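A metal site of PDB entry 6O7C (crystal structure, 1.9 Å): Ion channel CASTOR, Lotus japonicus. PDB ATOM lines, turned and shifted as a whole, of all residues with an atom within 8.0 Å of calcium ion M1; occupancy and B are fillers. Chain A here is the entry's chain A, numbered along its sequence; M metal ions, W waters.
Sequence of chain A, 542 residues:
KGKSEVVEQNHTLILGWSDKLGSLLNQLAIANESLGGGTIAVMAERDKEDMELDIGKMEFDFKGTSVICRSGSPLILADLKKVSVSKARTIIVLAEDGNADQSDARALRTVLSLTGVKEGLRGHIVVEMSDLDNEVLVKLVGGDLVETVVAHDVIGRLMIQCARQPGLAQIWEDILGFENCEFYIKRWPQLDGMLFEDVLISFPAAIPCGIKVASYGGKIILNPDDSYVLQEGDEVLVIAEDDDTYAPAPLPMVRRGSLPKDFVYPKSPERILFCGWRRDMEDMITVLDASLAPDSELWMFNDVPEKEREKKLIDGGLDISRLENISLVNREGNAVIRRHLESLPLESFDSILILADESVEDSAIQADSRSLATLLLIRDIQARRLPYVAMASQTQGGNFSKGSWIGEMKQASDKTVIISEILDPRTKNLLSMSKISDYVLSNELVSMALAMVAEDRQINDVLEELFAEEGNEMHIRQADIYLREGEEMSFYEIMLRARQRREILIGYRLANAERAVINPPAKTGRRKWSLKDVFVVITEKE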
ATOM      1  N   GLN A  27     -19.899 -11.093  27.877  1.00  0.00           N
ATOM      2  CA  GLN A  27     -21.267 -11.135  27.340  1.00  0.00           C
ATOM      3  C   GLN A  27     -22.298 -11.263  28.447  1.00  0.00           C
ATOM      4  O   GLN A  27     -23.359 -10.598  28.406  1.00  0.00           O
ATOM      5  CB  GLN A  27     -21.424 -12.309  26.352  1.00  0.00           C
ATOM      6  CG  GLN A  27     -20.648 -12.097  25.053  1.00  0.00           C
ATOM      7  CD  GLN A  27     -21.133 -10.851  24.294  1.00  0.00           C
ATOM      8  OE1 GLN A  27     -22.309 -10.636  24.204  1.00  0.00           O
ATOM      9  NE2 GLN A  27     -20.224 -10.050  23.789  1.00  0.00           N
ATOM     10  N   LEU A  28     -22.013 -12.127  29.425  1.00  0.00           N
ATOM     11  CA  LEU A  28     -22.947 -12.282  30.560  1.00  0.00           C
ATOM     12  C   LEU A  28     -23.006 -11.023  31.388  1.00  0.00           C
ATOM     13  O   LEU A  28     -24.085 -10.649  31.891  1.00  0.00           O
ATOM     14  CB  LEU A  28     -22.527 -13.507  31.418  1.00  0.00           C
ATOM     15  CG  LEU A  28     -22.737 -14.814  30.695  1.00  0.00           C
ATOM     16  CD1 LEU A  28     -21.917 -15.949  31.330  1.00  0.00           C
ATOM     17  CD2 LEU A  28     -24.273 -15.201  30.658  1.00  0.00           C
ATOM     18  N   ALA A  29     -21.897 -10.298  31.538  1.00  0.00           N
ATOM     19  CA  ALA A  29     -21.932  -9.048  32.283  1.00  0.00           C
ATOM     20  C   ALA A  29     -22.783  -8.040  31.543  1.00  0.00           C
ATOM     21  O   ALA A  29     -23.554  -7.274  32.172  1.00  0.00           O
ATOM     22  CB  ALA A  29     -20.505  -8.526  32.463  1.00  0.00           C
ATOM     23  N   ILE A  30     -22.659  -8.013  30.206  1.00  0.00           N
ATOM     24  CA  ILE A  30     -23.513  -7.099  29.412  1.00  0.00           C
ATOM     25  C   ILE A  30     -24.989  -7.464  29.588  1.00  0.00           C
ATOM     26  O   ILE A  30     -25.845  -6.599  29.855  1.00  0.00           O
ATOM     27  CB  ILE A  30     -23.082  -7.111  27.935  1.00  0.00           C
ATOM     28  CG1 ILE A  30     -21.609  -6.616  27.795  1.00  0.00           C
ATOM     29  CG2 ILE A  30     -24.045  -6.195  27.126  1.00  0.00           C
ATOM     30  CD1 ILE A  30     -21.034  -7.014  26.378  1.00  0.00           C
ATOM     31  N   ALA A  31     -25.304  -8.766  29.496  1.00  0.00           N
ATOM     32  CA  ALA A  31     -26.675  -9.218  29.651  1.00  0.00           C
ATOM     33  C   ALA A  31     -27.192  -8.864  31.058  1.00  0.00           C
ATOM     34  O   ALA A  31     -28.363  -8.508  31.233  1.00  0.00           O
ATOM     35  CB  ALA A  31     -26.803 -10.736  29.403  1.00  0.00           C
ATOM     36  N   ASN A  32     -26.356  -8.918  32.053  1.00  0.00           N
ATOM     37  CA  ASN A  32     -26.808  -8.675  33.427  1.00  0.00           C
ATOM     38  C   ASN A  32     -26.877  -7.196  33.768  1.00  0.00           C
ATOM     39  O   ASN A  32     -27.379  -6.889  34.853  1.00  0.00           O
ATOM     40  CB  ASN A  32     -25.893  -9.314  34.522  1.00  0.00           C
ATOM     41  CG  ASN A  32     -25.979 -10.841  34.580  1.00  0.00           C
ATOM     42  OD1 ASN A  32     -26.978 -11.450  34.186  1.00  0.00           O
ATOM     43  ND2 ASN A  32     -24.925 -11.479  35.154  1.00  0.00           N
ATOM     44  N   GLU A  33     -26.315  -6.299  32.917  1.00  0.00           N
ATOM     45  CA  GLU A  33     -26.180  -4.890  33.309  1.00  0.00           C
ATOM     46  C   GLU A  33     -27.538  -4.283  33.668  1.00  0.00           C
ATOM     47  O   GLU A  33     -27.665  -3.531  34.633  1.00  0.00           O
ATOM     48  CB  GLU A  33     -25.529  -4.099  32.190  1.00  0.00           C
ATOM     49  CG  GLU A  33     -25.224  -2.738  32.698  1.00  0.00           C
ATOM     50  CD  GLU A  33     -24.541  -1.833  31.679  1.00  0.00           C
ATOM     51  OE1 GLU A  33     -24.571  -2.089  30.467  1.00  0.00           O
ATOM     52  OE2 GLU A  33     -23.878  -0.887  32.156  1.00  0.00           O
ATOM     53  N   SER A  34     -28.571  -4.631  32.910  1.00  0.00           N
ATOM     54  CA  SER A  34     -29.883  -4.025  33.182  1.00  0.00           C
ATOM     55  C   SER A  34     -30.463  -4.428  34.536  1.00  0.00           C
ATOM     56  O   SER A  34     -31.423  -3.788  34.989  1.00  0.00           O
ATOM     57  CB  SER A  34     -30.848  -4.405  32.052  1.00  0.00           C
ATOM     58  OG  SER A  34     -31.012  -5.758  32.089  1.00  0.00           O
ATOM     59  N   LEU A  35     -29.930  -5.461  35.191  1.00  0.00           N
ATOM     60  CA  LEU A  35     -30.329  -5.875  36.533  1.00  0.00           C
ATOM     61  C   LEU A  35     -29.534  -5.180  37.615  1.00  0.00           C
ATOM     62  O   LEU A  35     -29.858  -5.328  38.806  1.00  0.00           O
ATOM     63  CB  LEU A  35     -30.129  -7.367  36.715  1.00  0.00           C
ATOM     64  CG  LEU A  35     -30.933  -8.242  35.765  1.00  0.00           C
ATOM     65  CD1 LEU A  35     -30.724  -9.788  35.929  1.00  0.00           C
ATOM     66  CD2 LEU A  35     -32.410  -7.836  35.897  1.00  0.00           C
ATOM     67  N   GLY A  36     -28.522  -4.413  37.219  1.00  0.00           N
ATOM     68  CA  GLY A  36     -27.551  -3.924  38.162  1.00  0.00           C
ATOM     69  C   GLY A  36     -26.423  -4.914  38.464  1.00  0.00           C
ATOM     70  O   GLY A  36     -25.678  -4.685  39.407  1.00  0.00           O
ATOM     71  N   PHE A 178     -24.592  -9.501  23.355  1.00  0.00           N
ATOM     72  CA  PHE A 178     -25.497  -8.584  24.040  1.00  0.00           C
ATOM     73  C   PHE A 178     -25.147  -7.111  23.871  1.00  0.00           C
ATOM     74  O   PHE A 178     -25.987  -6.257  24.211  1.00  0.00           O
ATOM     75  CB  PHE A 178     -25.622  -8.966  25.541  1.00  0.00           C
ATOM     76  CG  PHE A 178     -26.458 -10.172  25.734  1.00  0.00           C
ATOM     77  CD1 PHE A 178     -27.828 -10.072  25.762  1.00  0.00           C
ATOM     78  CD2 PHE A 178     -25.869 -11.480  25.790  1.00  0.00           C
ATOM     79  CE1 PHE A 178     -28.625 -11.172  25.905  1.00  0.00           C
ATOM     80  CE2 PHE A 178     -26.705 -12.605  25.899  1.00  0.00           C
ATOM     81  CZ  PHE A 178     -28.055 -12.470  25.955  1.00  0.00           C
ATOM     82  N   GLU A 182     -30.524  -7.592  20.196  1.00  0.00           N
ATOM     83  CA  GLU A 182     -30.567  -9.067  20.073  1.00  0.00           C
ATOM     84  C   GLU A 182     -32.012  -9.564  20.259  1.00  0.00           C
ATOM     85  O   GLU A 182     -32.954  -8.787  20.377  1.00  0.00           O
ATOM     86  CB  GLU A 182     -29.578  -9.740  21.064  1.00  0.00           C
ATOM     87  CG  GLU A 182     -29.854  -9.298  22.556  1.00  0.00           C
ATOM     88  CD  GLU A 182     -29.121  -7.957  22.940  1.00  0.00           C
ATOM     89  OE1 GLU A 182     -28.300  -7.332  22.196  1.00  0.00           O
ATOM     90  OE2 GLU A 182     -29.548  -7.439  23.990  1.00  0.00           O
ATOM     91  N   TYR A 184     -35.303 -11.259  22.048  1.00  0.00           N
ATOM     92  CA  TYR A 184     -35.946 -11.447  23.328  1.00  0.00           C
ATOM     93  C   TYR A 184     -37.304 -12.062  23.084  1.00  0.00           C
ATOM     94  O   TYR A 184     -37.964 -11.749  22.100  1.00  0.00           O
ATOM     95  CB  TYR A 184     -36.112 -10.154  24.137  1.00  0.00           C
ATOM     96  CG  TYR A 184     -34.735  -9.673  24.614  1.00  0.00           C
ATOM     97  CD1 TYR A 184     -34.108 -10.258  25.721  1.00  0.00           C
ATOM     98  CD2 TYR A 184     -34.057  -8.721  23.918  1.00  0.00           C
ATOM     99  CE1 TYR A 184     -32.841  -9.863  26.115  1.00  0.00           C
ATOM    100  CE2 TYR A 184     -32.809  -8.289  24.339  1.00  0.00           C
ATOM    101  CZ  TYR A 184     -32.212  -8.886  25.416  1.00  0.00           C
ATOM    102  OH  TYR A 184     -30.915  -8.488  25.799  1.00  0.00           O
ATOM    103  N   GLU A 241     -33.121  -3.649  22.149  1.00  0.00           N
ATOM    104  CA  GLU A 241     -31.776  -3.336  22.686  1.00  0.00           C
ATOM    105  C   GLU A 241     -31.492  -4.122  23.961  1.00  0.00           C
ATOM    106  O   GLU A 241     -30.342  -4.396  24.269  1.00  0.00           O
ATOM    107  CB  GLU A 241     -31.629  -1.816  22.968  1.00  0.00           C
ATOM    108  CG  GLU A 241     -30.223  -1.371  23.442  1.00  0.00           C
ATOM    109  CD  GLU A 241     -30.103   0.095  23.972  1.00  0.00           C
ATOM    110  OE1 GLU A 241     -31.087   0.867  23.913  1.00  0.00           O
ATOM    111  OE2 GLU A 241     -29.018   0.450  24.526  1.00  0.00           O
ATOM    112  N   ASP A 242     -32.499  -4.397  24.817  1.00  0.00           N
ATOM    113  CA  ASP A 242     -32.230  -5.132  26.055  1.00  0.00           C
ATOM    114  C   ASP A 242     -33.582  -5.726  26.448  1.00  0.00           C
ATOM    115  O   ASP A 242     -34.593  -5.462  25.780  1.00  0.00           O
ATOM    116  CB  ASP A 242     -31.680  -4.180  27.139  1.00  0.00           C
ATOM    117  CG  ASP A 242     -30.765  -4.890  28.157  1.00  0.00           C
ATOM    118  OD1 ASP A 242     -30.918  -6.105  28.316  1.00  0.00           O
ATOM    119  OD2 ASP A 242     -29.850  -4.215  28.695  1.00  0.00           O
ATOM    120  N   ASP A 243     -33.599  -6.541  27.517  1.00  0.00           N
ATOM    121  CA  ASP A 243     -34.840  -7.218  27.807  1.00  0.00           C
ATOM    122  C   ASP A 243     -35.922  -6.247  28.296  1.00  0.00           C
ATOM    123  O   ASP A 243     -37.118  -6.623  28.295  1.00  0.00           O
ATOM    124  CB  ASP A 243     -34.687  -8.348  28.880  1.00  0.00           C
ATOM    125  CG  ASP A 243     -33.993  -7.859  30.139  1.00  0.00           C
ATOM    126  OD1 ASP A 243     -32.770  -7.583  30.100  1.00  0.00           O
ATOM    127  OD2 ASP A 243     -34.705  -7.462  31.119  1.00  0.00           O
ATOM    128  N   ASP A 244     -35.552  -5.037  28.757  1.00  0.00           N
ATOM    129  CA  ASP A 244     -36.489  -4.154  29.437  1.00  0.00           C
ATOM    130  C   ASP A 244     -36.649  -2.798  28.732  1.00  0.00           C
ATOM    131  O   ASP A 244     -37.076  -1.815  29.364  1.00  0.00           O
ATOM    132  CB  ASP A 244     -36.025  -3.966  30.883  1.00  0.00           C
ATOM    133  CG  ASP A 244     -34.653  -3.235  31.003  1.00  0.00           C
ATOM    134  OD1 ASP A 244     -33.938  -2.964  29.973  1.00  0.00           O
ATOM    135  OD2 ASP A 244     -34.290  -2.841  32.145  1.00  0.00           O
ATOM    136  N   THR A 245     -36.232  -2.682  27.471  1.00  0.00           N
ATOM    137  CA  THR A 245     -36.217  -1.373  26.816  1.00  0.00           C
ATOM    138  C   THR A 245     -37.410  -1.176  25.910  1.00  0.00           C
ATOM    139  O   THR A 245     -37.563  -0.086  25.325  1.00  0.00           O
ATOM    140  CB  THR A 245     -34.937  -1.200  25.983  1.00  0.00           C
ATOM    141  OG1 THR A 245     -34.855  -2.304  25.090  1.00  0.00           O
ATOM    142  CG2 THR A 245     -33.698  -1.140  26.875  1.00  0.00           C
ATOM    143  N   GLU A 455     -28.911 -17.284  28.380  1.00  0.00           N
ATOM    144  CA  GLU A 455     -29.915 -16.350  28.876  1.00  0.00           C
ATOM    145  C   GLU A 455     -31.338 -16.795  28.536  1.00  0.00           C
ATOM    146  O   GLU A 455     -32.248 -16.532  29.320  1.00  0.00           O
ATOM    147  CB  GLU A 455     -29.666 -14.917  28.312  1.00  0.00           C
ATOM    148  CG  GLU A 455     -28.409 -14.381  29.038  1.00  0.00           C
ATOM    149  CD  GLU A 455     -28.671 -14.083  30.490  1.00  0.00           C
ATOM    150  OE1 GLU A 455     -29.413 -13.132  30.795  1.00  0.00           O
ATOM    151  OE2 GLU A 455     -28.226 -14.897  31.347  1.00  0.00           O
HETATM  152 CA    CA M   1     -30.410  -7.472  30.361  1.00  0.00          CA
HETATM  153 CA    CA M   2     -28.173  -5.451  23.983  1.00  0.00          CA
HETATM  154  O   HOH W   1     -31.000  -9.193  31.895  1.00  0.00           O
HETATM  155  O   HOH W   2     -30.115  -8.924  28.496  1.00  0.00           O
HETATM  156  O   HOH W   3     -28.551  -5.849  30.266  1.00  0.00           O
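The side-chain carboxylate (OD1) of Asp 242 lies close to the side-chain hydroxyl (OH) of Tyr 184, at 3.5 Å. OG1 of Thr 245 lies within hydrogen-bond range of N of Asp 242, at 3.2 Å.
Four residues have an atom within 4 Å of calcium ion M1: Ala 31, Ser 34, Asp 242 and Asp 243. The nearest printed residue that does not touch calcium ion M1 is Asn 32 (4.6 Å).
Calcium ion M1 is bound by OD1 of Asp 243 (2.4 Å), water W1 (2.4 Å), water W2 (2.4 Å), O of Ala 31 (2.5 Å), water W3 (2.5 Å), OG of Ser 34 (2.5 Å) and OD1 of Asp 242 (2.5 Å).
Water W3 lies within hydrogen-bond range of the side-chain carboxylate of Asp 242 (2.6 Å), the backbone carbonyl oxygen of Ile 30 (2.8 Å), the backbone NH of Ser 34 (2.9 Å) and the backbone NH of Glu 33 (3.5 Å).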
